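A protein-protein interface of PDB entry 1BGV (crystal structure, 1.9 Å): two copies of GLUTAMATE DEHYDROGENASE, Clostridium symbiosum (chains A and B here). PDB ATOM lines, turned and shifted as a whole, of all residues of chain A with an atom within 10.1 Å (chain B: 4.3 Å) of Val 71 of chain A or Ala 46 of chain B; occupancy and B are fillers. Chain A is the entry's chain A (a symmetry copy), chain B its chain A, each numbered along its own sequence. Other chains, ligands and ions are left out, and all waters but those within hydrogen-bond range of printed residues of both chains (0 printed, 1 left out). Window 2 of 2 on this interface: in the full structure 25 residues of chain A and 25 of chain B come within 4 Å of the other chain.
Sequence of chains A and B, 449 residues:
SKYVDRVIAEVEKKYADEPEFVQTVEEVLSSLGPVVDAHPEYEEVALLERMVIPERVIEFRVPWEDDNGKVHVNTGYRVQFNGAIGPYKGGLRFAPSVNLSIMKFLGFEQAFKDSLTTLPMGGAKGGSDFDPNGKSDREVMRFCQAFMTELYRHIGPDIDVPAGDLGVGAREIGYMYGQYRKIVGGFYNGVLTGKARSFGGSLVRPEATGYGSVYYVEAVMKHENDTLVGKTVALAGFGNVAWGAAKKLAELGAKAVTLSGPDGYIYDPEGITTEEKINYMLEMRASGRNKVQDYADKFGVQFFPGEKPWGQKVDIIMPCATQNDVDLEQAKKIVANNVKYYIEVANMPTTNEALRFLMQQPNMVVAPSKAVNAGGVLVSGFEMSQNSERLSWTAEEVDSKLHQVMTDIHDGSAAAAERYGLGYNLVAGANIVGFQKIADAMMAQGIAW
O of Arg 50 of chain B sits at hydrogen-bond distance from NE of Arg 61 of chain A (2.9 Å).
OE1 of Glu 49 of chain B is in hydrogen-bond range of OH of Tyr 3 of chain B, 2.6 Å away.
O of Val 45 of chain B sits at hydrogen-bond distance from NH2 of Arg 50 of chain B, at 2.9 Å.
Pro 63 of chain A touches Arg 50 of chain B (CG to CD, 3.8 Å).
Val 71 of chain A touches Val 45 of chain B (CG1 to O, 3.6 Å).
Ala 46 of chain B touches Val 71 of chain A (CB to O, 3.7 Å).
Val 73 of chain A touches Glu 49 of chain B.
Arg 50 of chain B touches Val 73 of chain A (CG to CG2, 3.7 Å).
Printed residues of chain B within 4 Å of Arg 61 of chain A: Arg 50 (2.9 Å).
Of the printed residues of chain B, Pro 63 of chain A touches Arg 50 (3.8 Å).
Glu 65 of chain A touches none of the printed residues of chain B.
Val 71 of chain A touches just these residues of chain B: Val 45 and Ala 46.
Of the printed residues of chain B, Val 73 of chain A touches Glu 49 and Arg 50.
Glu 139 of chain A touches none of the printed residues of chain B.
Printed residues of chain A within 4 Å of Val 45 of chain B: Val 71.
Ala 46 of chain B touches just one residue of chain A: Val 71 (3.7 Å).
Glu 49 of chain B touches just one residue of chain A: Val 73 (3.9 Å).
Printed residues of chain A within 4 Å of Arg 50 of chain B: Arg 61, Pro 63 and Val 73.
The nearest residue of chain B that does not touch Val 71 of chain A is Glu 44 of chain B (4.1 Å).
The nearest residue of chain A that does not touch Ala 46 of chain B is Val 73 of chain A (4.4 Å).
The nearest printed residue of chain B that does not touch Arg 61 of chain A is Glu 49 of chain B (5.7 Å).
Of the 19 printed residues of chain A, 4 touch a printed residue of chain B.
Hydrophobic or aromatic side chains of chain A within 4 Å of the printed part of chain B: Pro 63, Val 71 and Val 73.
Among the printed residues, no Asp or Glu carboxylate lies within 4 Å of a Lys or Arg side-chain nitrogen of the other chain.
No position is printed for both chains.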
ATOM      1  N   ARG A  61      37.132   0.663  -2.001  1.00  0.00           N
ATOM      2  CA  ARG A  61      36.316  -0.036  -3.023  1.00  0.00           C
ATOM      3  C   ARG A  61      35.515  -1.126  -2.332  1.00  0.00           C
ATOM      4  O   ARG A  61      36.077  -1.809  -1.476  1.00  0.00           O
ATOM      5  CB  ARG A  61      37.280  -0.698  -4.018  1.00  0.00           C
ATOM      6  CG  ARG A  61      36.558  -1.217  -5.205  1.00  0.00           C
ATOM      7  CD  ARG A  61      37.412  -1.952  -6.171  1.00  0.00           C
ATOM      8  NE  ARG A  61      38.577  -1.258  -6.639  1.00  0.00           N
ATOM      9  CZ  ARG A  61      39.615  -1.881  -7.197  1.00  0.00           C
ATOM     10  NH1 ARG A  61      39.687  -3.236  -7.248  1.00  0.00           N
ATOM     11  NH2 ARG A  61      40.659  -1.162  -7.636  1.00  0.00           N
ATOM     12  N   VAL A  62      34.252  -1.367  -2.728  1.00  0.00           N
ATOM     13  CA  VAL A  62      33.494  -2.485  -2.144  1.00  0.00           C
ATOM     14  C   VAL A  62      32.791  -3.266  -3.265  1.00  0.00           C
ATOM     15  O   VAL A  62      31.670  -2.928  -3.579  1.00  0.00           O
ATOM     16  CB  VAL A  62      32.444  -2.046  -1.102  1.00  0.00           C
ATOM     17  CG1 VAL A  62      31.900  -3.312  -0.304  1.00  0.00           C
ATOM     18  CG2 VAL A  62      33.048  -1.014  -0.066  1.00  0.00           C
ATOM     19  N   PRO A  63      33.447  -4.281  -3.829  1.00  0.00           N
ATOM     20  CA  PRO A  63      32.771  -5.105  -4.852  1.00  0.00           C
ATOM     21  C   PRO A  63      31.976  -6.121  -4.072  1.00  0.00           C
ATOM     22  O   PRO A  63      32.391  -6.602  -3.009  1.00  0.00           O
ATOM     23  CB  PRO A  63      33.882  -5.860  -5.606  1.00  0.00           C
ATOM     24  CG  PRO A  63      35.243  -5.340  -4.979  1.00  0.00           C
ATOM     25  CD  PRO A  63      34.868  -4.660  -3.646  1.00  0.00           C
ATOM     26  N   TRP A  64      30.836  -6.481  -4.610  1.00  0.00           N
ATOM     27  CA  TRP A  64      30.048  -7.527  -3.982  1.00  0.00           C
ATOM     28  C   TRP A  64      29.121  -8.178  -5.039  1.00  0.00           C
ATOM     29  O   TRP A  64      28.903  -7.616  -6.124  1.00  0.00           O
ATOM     30  CB  TRP A  64      29.248  -6.948  -2.869  1.00  0.00           C
ATOM     31  CG  TRP A  64      28.338  -5.881  -3.336  1.00  0.00           C
ATOM     32  CD1 TRP A  64      28.631  -4.561  -3.517  1.00  0.00           C
ATOM     33  CD2 TRP A  64      26.923  -6.028  -3.564  1.00  0.00           C
ATOM     34  NE1 TRP A  64      27.460  -3.877  -3.820  1.00  0.00           N
ATOM     35  CE2 TRP A  64      26.421  -4.774  -3.919  1.00  0.00           C
ATOM     36  CE3 TRP A  64      26.042  -7.119  -3.502  1.00  0.00           C
ATOM     37  CZ2 TRP A  64      25.066  -4.580  -4.286  1.00  0.00           C
ATOM     38  CZ3 TRP A  64      24.683  -6.921  -3.877  1.00  0.00           C
ATOM     39  CH2 TRP A  64      24.208  -5.666  -4.224  1.00  0.00           C
ATOM     40  N   GLU A  65      28.599  -9.366  -4.743  1.00  0.00           N
ATOM     41  CA  GLU A  65      27.787 -10.078  -5.771  1.00  0.00           C
ATOM     42  C   GLU A  65      26.327 -10.229  -5.324  1.00  0.00           C
ATOM     43  O   GLU A  65      26.069 -10.509  -4.109  1.00  0.00           O
ATOM     44  CB  GLU A  65      28.440 -11.422  -6.166  1.00  0.00           C
ATOM     45  CG  GLU A  65      27.792 -12.614  -5.614  1.00  0.00           C
ATOM     46  CD  GLU A  65      28.507 -13.886  -6.032  1.00  0.00           C
ATOM     47  OE1 GLU A  65      28.446 -14.264  -7.233  1.00  0.00           O
ATOM     48  OE2 GLU A  65      29.169 -14.487  -5.141  1.00  0.00           O
ATOM     49  N   ASP A  66      25.382  -9.973  -6.264  1.00  0.00           N
ATOM     50  CA  ASP A  66      23.951 -10.072  -5.898  1.00  0.00           C
ATOM     51  C   ASP A  66      23.421 -11.504  -5.995  1.00  0.00           C
ATOM     52  O   ASP A  66      24.166 -12.441  -6.394  1.00  0.00           O
ATOM     53  CB  ASP A  66      23.051  -9.097  -6.669  1.00  0.00           C
ATOM     54  CG  ASP A  66      22.933  -9.436  -8.163  1.00  0.00           C
ATOM     55  OD1 ASP A  66      23.210 -10.563  -8.652  1.00  0.00           O
ATOM     56  OD2 ASP A  66      22.600  -8.465  -8.853  1.00  0.00           O
ATOM     57  N   ASP A  67      22.147 -11.672  -5.631  1.00  0.00           N
ATOM     58  CA  ASP A  67      21.524 -13.019  -5.601  1.00  0.00           C
ATOM     59  C   ASP A  67      21.561 -13.678  -6.981  1.00  0.00           C
ATOM     60  O   ASP A  67      21.551 -14.887  -7.076  1.00  0.00           O
ATOM     61  CB  ASP A  67      20.101 -12.953  -5.060  1.00  0.00           C
ATOM     62  CG  ASP A  67      20.065 -12.795  -3.585  1.00  0.00           C
ATOM     63  OD1 ASP A  67      21.128 -12.974  -2.970  1.00  0.00           O
ATOM     64  OD2 ASP A  67      19.029 -12.461  -2.983  1.00  0.00           O
ATOM     65  N   ASN A  68      21.663 -12.872  -8.048  1.00  0.00           N
ATOM     66  CA  ASN A  68      21.728 -13.379  -9.417  1.00  0.00           C
ATOM     67  C   ASN A  68      23.132 -13.568  -9.889  1.00  0.00           C
ATOM     68  O   ASN A  68      23.269 -13.957 -11.023  1.00  0.00           O
ATOM     69  CB  ASN A  68      21.082 -12.389 -10.378  1.00  0.00           C
ATOM     70  CG  ASN A  68      19.593 -12.231 -10.112  1.00  0.00           C
ATOM     71  OD1 ASN A  68      19.067 -11.118 -10.059  1.00  0.00           O
ATOM     72  ND2 ASN A  68      18.935 -13.348  -9.815  1.00  0.00           N
ATOM     73  N   GLY A  69      24.163 -13.297  -9.068  1.00  0.00           N
ATOM     74  CA  GLY A  69      25.547 -13.528  -9.527  1.00  0.00           C
ATOM     75  C   GLY A  69      26.114 -12.304 -10.264  1.00  0.00           C
ATOM     76  O   GLY A  69      27.249 -12.324 -10.715  1.00  0.00           O
ATOM     77  N   LYS A  70      25.380 -11.201 -10.290  1.00  0.00           N
ATOM     78  CA  LYS A  70      25.918 -10.028 -10.937  1.00  0.00           C
ATOM     79  C   LYS A  70      26.809  -9.303  -9.923  1.00  0.00           C
ATOM     80  O   LYS A  70      26.446  -9.203  -8.741  1.00  0.00           O
ATOM     81  CB  LYS A  70      24.765  -9.117 -11.347  1.00  0.00           C
ATOM     82  CG  LYS A  70      25.236  -7.744 -11.695  1.00  0.00           C
ATOM     83  CD  LYS A  70      24.175  -6.976 -12.448  1.00  0.00           C
ATOM     84  CE  LYS A  70      24.785  -5.811 -13.268  1.00  0.00           C
ATOM     85  NZ  LYS A  70      23.959  -4.534 -13.322  1.00  0.00           N
ATOM     86  N   VAL A  71      27.932  -8.792 -10.440  1.00  0.00           N
ATOM     87  CA  VAL A  71      28.871  -8.045  -9.606  1.00  0.00           C
ATOM     88  C   VAL A  71      28.599  -6.547  -9.581  1.00  0.00           C
ATOM     89  O   VAL A  71      28.464  -5.907 -10.618  1.00  0.00           O
ATOM     90  CB  VAL A  71      30.292  -8.365 -10.045  1.00  0.00           C
ATOM     91  CG1 VAL A  71      31.334  -7.609  -9.200  1.00  0.00           C
ATOM     92  CG2 VAL A  71      30.500  -9.844  -9.869  1.00  0.00           C
ATOM     93  N   HIS A  72      28.428  -6.001  -8.385  1.00  0.00           N
ATOM     94  CA  HIS A  72      28.254  -4.574  -8.173  1.00  0.00           C
ATOM     95  C   HIS A  72      29.454  -3.949  -7.416  1.00  0.00           C
ATOM     96  O   HIS A  72      30.224  -4.625  -6.746  1.00  0.00           O
ATOM     97  CB  HIS A  72      27.058  -4.324  -7.326  1.00  0.00           C
ATOM     98  CG  HIS A  72      25.825  -4.889  -7.921  1.00  0.00           C
ATOM     99  ND1 HIS A  72      24.991  -4.129  -8.706  1.00  0.00           N
ATOM    100  CD2 HIS A  72      25.365  -6.157  -8.000  1.00  0.00           C
ATOM    101  CE1 HIS A  72      24.013  -4.881  -9.164  1.00  0.00           C
ATOM    102  NE2 HIS A  72      24.216  -6.116  -8.761  1.00  0.00           N
ATOM    103  N   VAL A  73      29.666  -2.666  -7.635  1.00  0.00           N
ATOM    104  CA  VAL A  73      30.778  -1.989  -6.972  1.00  0.00           C
ATOM    105  C   VAL A  73      30.308  -0.751  -6.254  1.00  0.00           C
ATOM    106  O   VAL A  73      29.728   0.096  -6.920  1.00  0.00           O
ATOM    107  CB  VAL A  73      31.951  -1.632  -7.939  1.00  0.00           C
ATOM    108  CG1 VAL A  73      33.214  -1.458  -7.086  1.00  0.00           C
ATOM    109  CG2 VAL A  73      32.257  -2.735  -8.877  1.00  0.00           C
ATOM    110  N   ASN A  74      30.583  -0.601  -4.953  1.00  0.00           N
ATOM    111  CA  ASN A  74      30.255   0.636  -4.251  1.00  0.00           C
ATOM    112  C   ASN A  74      31.484   1.151  -3.557  1.00  0.00           C
ATOM    113  O   ASN A  74      32.556   0.574  -3.682  1.00  0.00           O
ATOM    114  CB  ASN A  74      29.136   0.424  -3.249  1.00  0.00           C
ATOM    115  CG  ASN A  74      27.799   0.213  -3.953  1.00  0.00           C
ATOM    116  OD1 ASN A  74      27.425  -0.912  -4.251  1.00  0.00           O
ATOM    117  ND2 ASN A  74      27.145   1.316  -4.337  1.00  0.00           N
ATOM    118  N   LYS A 135      17.119  -4.685  -1.650  1.00  0.00           N
ATOM    119  CA  LYS A 135      18.126  -5.753  -1.706  1.00  0.00           C
ATOM    120  C   LYS A 135      17.581  -6.925  -0.879  1.00  0.00           C
ATOM    121  O   LYS A 135      16.890  -6.666   0.125  1.00  0.00           O
ATOM    122  CB  LYS A 135      19.395  -5.237  -1.001  1.00  0.00           C
ATOM    123  CG  LYS A 135      19.897  -3.969  -1.678  1.00  0.00           C
ATOM    124  CD  LYS A 135      20.492  -4.421  -2.970  1.00  0.00           C
ATOM    125  CE  LYS A 135      21.241  -3.296  -3.759  1.00  0.00           C
ATOM    126  NZ  LYS A 135      20.384  -2.168  -4.194  1.00  0.00           N
ATOM    127  N   GLU A 139      21.651 -10.377   0.191  1.00  0.00           N
ATOM    128  CA  GLU A 139      22.470  -9.389  -0.529  1.00  0.00           C
ATOM    129  C   GLU A 139      23.065  -8.389   0.484  1.00  0.00           C
ATOM    130  O   GLU A 139      24.210  -8.018   0.390  1.00  0.00           O
ATOM    131  CB  GLU A 139      21.604  -8.621  -1.547  1.00  0.00           C
ATOM    132  CG  GLU A 139      21.568  -9.467  -2.839  1.00  0.00           C
ATOM    133  CD  GLU A 139      20.448  -9.062  -3.841  1.00  0.00           C
ATOM    134  OE1 GLU A 139      19.499  -8.312  -3.454  1.00  0.00           O
ATOM    135  OE2 GLU A 139      20.506  -9.613  -4.959  1.00  0.00           O
ATOM    136  N   ARG A 142      26.076 -10.097   2.151  1.00  0.00           N
ATOM    137  CA  ARG A 142      27.312 -10.172   1.435  1.00  0.00           C
ATOM    138  C   ARG A 142      27.927  -8.791   1.376  1.00  0.00           C
ATOM    139  O   ARG A 142      29.151  -8.681   1.363  1.00  0.00           O
ATOM    140  CB  ARG A 142      27.096 -10.728   0.032  1.00  0.00           C
ATOM    141  CG  ARG A 142      26.524 -12.165   0.064  1.00  0.00           C
ATOM    142  CD  ARG A 142      26.894 -13.084  -1.121  1.00  0.00           C
ATOM    143  NE  ARG A 142      25.979 -12.786  -2.111  1.00  0.00           N
ATOM    144  CZ  ARG A 142      24.718 -13.161  -2.233  1.00  0.00           C
ATOM    145  NH1 ARG A 142      24.173 -14.278  -1.788  1.00  0.00           N
ATOM    146  NH2 ARG A 142      24.055 -12.422  -3.081  1.00  0.00           N
ATOM    147  N   PHE A 143      27.105  -7.742   1.293  1.00  0.00           N
ATOM    148  CA  PHE A 143      27.639  -6.372   1.168  1.00  0.00           C
ATOM    149  C   PHE A 143      28.349  -6.042   2.464  1.00  0.00           C
ATOM    150  O   PHE A 143      29.488  -5.617   2.456  1.00  0.00           O
ATOM    151  CB  PHE A 143      26.540  -5.309   0.969  1.00  0.00           C
ATOM    152  CG  PHE A 143      27.112  -3.918   0.909  1.00  0.00           C
ATOM    153  CD1 PHE A 143      27.840  -3.568  -0.202  1.00  0.00           C
ATOM    154  CD2 PHE A 143      27.094  -3.077   2.046  1.00  0.00           C
ATOM    155  CE1 PHE A 143      28.501  -2.356  -0.237  1.00  0.00           C
ATOM    156  CE2 PHE A 143      27.767  -1.883   2.048  1.00  0.00           C
ATOM    157  CZ  PHE A 143      28.496  -1.537   0.905  1.00  0.00           C
ATOM    158  N   ALA A 146      31.692  -7.780   2.689  1.00  0.00           N
ATOM    159  CA  ALA A 146      32.746  -7.238   1.849  1.00  0.00           C
ATOM    160  C   ALA A 146      33.164  -5.867   2.421  1.00  0.00           C
ATOM    161  O   ALA A 146      34.368  -5.561   2.370  1.00  0.00           O
ATOM    162  CB  ALA A 146      32.274  -7.047   0.380  1.00  0.00           C
ATOM    163  N   TYR B   3      30.540  -1.253 -23.605  1.00  0.00           N
ATOM    164  CA  TYR B   3      30.864  -1.437 -22.169  1.00  0.00           C
ATOM    165  C   TYR B   3      31.819  -0.306 -21.745  1.00  0.00           C
ATOM    166  O   TYR B   3      31.628   0.440 -20.778  1.00  0.00           O
ATOM    167  CB  TYR B   3      31.557  -2.799 -22.040  1.00  0.00           C
ATOM    168  CG  TYR B   3      32.062  -3.127 -20.629  1.00  0.00           C
ATOM    169  CD1 TYR B   3      31.468  -2.559 -19.481  1.00  0.00           C
ATOM    170  CD2 TYR B   3      33.146  -3.985 -20.463  1.00  0.00           C
ATOM    171  CE1 TYR B   3      31.919  -2.897 -18.195  1.00  0.00           C
ATOM    172  CE2 TYR B   3      33.569  -4.396 -19.180  1.00  0.00           C
ATOM    173  CZ  TYR B   3      32.998  -3.798 -18.073  1.00  0.00           C
ATOM    174  OH  TYR B   3      33.421  -4.175 -16.821  1.00  0.00           O
ATOM    175  N   TYR B  42      35.241 -10.034 -19.006  1.00  0.00           N
ATOM    176  CA  TYR B  42      35.509  -8.879 -18.136  1.00  0.00           C
ATOM    177  C   TYR B  42      34.229  -8.230 -17.638  1.00  0.00           C
ATOM    178  O   TYR B  42      34.112  -7.788 -16.489  1.00  0.00           O
ATOM    179  CB  TYR B  42      36.331  -7.797 -18.829  1.00  0.00           C
ATOM    180  CG  TYR B  42      37.645  -8.271 -19.299  1.00  0.00           C
ATOM    181  CD1 TYR B  42      38.241  -9.430 -18.764  1.00  0.00           C
ATOM    182  CD2 TYR B  42      38.380  -7.475 -20.158  1.00  0.00           C
ATOM    183  CE1 TYR B  42      39.555  -9.782 -19.109  1.00  0.00           C
ATOM    184  CE2 TYR B  42      39.654  -7.819 -20.530  1.00  0.00           C
ATOM    185  CZ  TYR B  42      40.230  -8.973 -20.031  1.00  0.00           C
ATOM    186  OH  TYR B  42      41.504  -9.271 -20.500  1.00  0.00           O
ATOM    187  N   GLU B  43      33.271  -8.063 -18.530  1.00  0.00           N
ATOM    188  CA  GLU B  43      32.110  -7.324 -18.139  1.00  0.00           C
ATOM    189  C   GLU B  43      31.303  -8.096 -17.103  1.00  0.00           C
ATOM    190  O   GLU B  43      30.585  -7.547 -16.204  1.00  0.00           O
ATOM    191  CB  GLU B  43      31.256  -6.959 -19.366  1.00  0.00           C
ATOM    192  CG  GLU B  43      29.938  -6.275 -18.946  1.00  0.00           C
ATOM    193  CD  GLU B  43      29.160  -5.638 -20.123  1.00  0.00           C
ATOM    194  OE1 GLU B  43      29.473  -6.058 -21.245  1.00  0.00           O
ATOM    195  OE2 GLU B  43      28.256  -4.763 -19.934  1.00  0.00           O
ATOM    196  N   GLU B  44      31.416  -9.397 -17.187  1.00  0.00           N
ATOM    197  CA  GLU B  44      30.588 -10.119 -16.253  1.00  0.00           C
ATOM    198  C   GLU B  44      31.019  -9.934 -14.825  1.00  0.00           C
ATOM    199  O   GLU B  44      30.212 -10.140 -13.948  1.00  0.00           O
ATOM    200  CB  GLU B  44      30.635 -11.595 -16.567  1.00  0.00           C
ATOM    201  CG  GLU B  44      29.889 -11.994 -17.814  1.00  0.00           C
ATOM    202  CD  GLU B  44      30.457 -13.278 -18.376  1.00  0.00           C
ATOM    203  OE1 GLU B  44      31.183 -13.959 -17.598  1.00  0.00           O
ATOM    204  OE2 GLU B  44      30.248 -13.569 -19.599  1.00  0.00           O
ATOM    205  N   VAL B  45      32.305  -9.681 -14.580  1.00  0.00           N
ATOM    206  CA  VAL B  45      32.763  -9.519 -13.186  1.00  0.00           C
ATOM    207  C   VAL B  45      32.966  -8.039 -12.883  1.00  0.00           C
ATOM    208  O   VAL B  45      33.665  -7.680 -11.915  1.00  0.00           O
ATOM    209  CB  VAL B  45      34.000 -10.338 -12.890  1.00  0.00           C
ATOM    210  CG1 VAL B  45      33.668 -11.823 -12.976  1.00  0.00           C
ATOM    211  CG2 VAL B  45      35.096 -10.055 -13.875  1.00  0.00           C
ATOM    212  N   ALA B  46      32.386  -7.195 -13.750  1.00  0.00           N
ATOM    213  CA  ALA B  46      32.480  -5.748 -13.568  1.00  0.00           C
ATOM    214  C   ALA B  46      33.950  -5.299 -13.376  1.00  0.00           C
ATOM    215  O   ALA B  46      34.322  -4.479 -12.505  1.00  0.00           O
ATOM    216  CB  ALA B  46      31.694  -5.366 -12.387  1.00  0.00           C
ATOM    217  N   LEU B  47      34.791  -5.828 -14.227  1.00  0.00           N
ATOM    218  CA  LEU B  47      36.202  -5.500 -14.095  1.00  0.00           C
ATOM    219  C   LEU B  47      36.494  -3.996 -14.199  1.00  0.00           C
ATOM    220  O   LEU B  47      37.331  -3.483 -13.491  1.00  0.00           O
ATOM    221  CB  LEU B  47      37.000  -6.272 -15.181  1.00  0.00           C
ATOM    222  CG  LEU B  47      38.506  -6.038 -15.099  1.00  0.00           C
ATOM    223  CD1 LEU B  47      39.076  -6.665 -13.773  1.00  0.00           C
ATOM    224  CD2 LEU B  47      39.258  -6.553 -16.294  1.00  0.00           C
ATOM    225  N   LEU B  48      35.977  -3.328 -15.221  1.00  0.00           N
ATOM    226  CA  LEU B  48      36.324  -1.911 -15.409  1.00  0.00           C
ATOM    227  C   LEU B  48      35.741  -1.095 -14.323  1.00  0.00           C
ATOM    228  O   LEU B  48      36.368  -0.153 -13.885  1.00  0.00           O
ATOM    229  CB  LEU B  48      35.829  -1.379 -16.785  1.00  0.00           C
ATOM    230  CG  LEU B  48      36.478  -2.035 -18.015  1.00  0.00           C
ATOM    231  CD1 LEU B  48      35.911  -1.362 -19.210  1.00  0.00           C
ATOM    232  CD2 LEU B  48      37.982  -1.958 -18.069  1.00  0.00           C
ATOM    233  N   GLU B  49      34.523  -1.443 -13.874  1.00  0.00           N
ATOM    234  CA  GLU B  49      33.950  -0.673 -12.810  1.00  0.00           C
ATOM    235  C   GLU B  49      34.816  -0.785 -11.559  1.00  0.00           C
ATOM    236  O   GLU B  49      34.914   0.165 -10.801  1.00  0.00           O
ATOM    237  CB  GLU B  49      32.536  -1.112 -12.463  1.00  0.00           C
ATOM    238  CG  GLU B  49      31.507  -0.927 -13.580  1.00  0.00           C
ATOM    239  CD  GLU B  49      31.436  -2.168 -14.489  1.00  0.00           C
ATOM    240  OE1 GLU B  49      32.485  -2.828 -14.793  1.00  0.00           O
ATOM    241  OE2 GLU B  49      30.335  -2.424 -15.031  1.00  0.00           O
ATOM    242  N   ARG B  50      35.338  -1.965 -11.265  1.00  0.00           N
ATOM    243  CA  ARG B  50      36.282  -2.118 -10.135  1.00  0.00           C
ATOM    244  C   ARG B  50      37.581  -1.277 -10.320  1.00  0.00           C
ATOM    245  O   ARG B  50      38.036  -0.616  -9.399  1.00  0.00           O
ATOM    246  CB  ARG B  50      36.629  -3.626 -10.002  1.00  0.00           C
ATOM    247  CG  ARG B  50      35.492  -4.373  -9.299  1.00  0.00           C
ATOM    248  CD  ARG B  50      36.172  -5.569  -8.705  1.00  0.00           C
ATOM    249  NE  ARG B  50      36.028  -6.562  -9.696  1.00  0.00           N
ATOM    250  CZ  ARG B  50      36.788  -7.629  -9.982  1.00  0.00           C
ATOM    251  NH1 ARG B  50      37.862  -8.031  -9.330  1.00  0.00           N
ATOM    252  NH2 ARG B  50      36.362  -8.397 -10.991  1.00  0.00           N
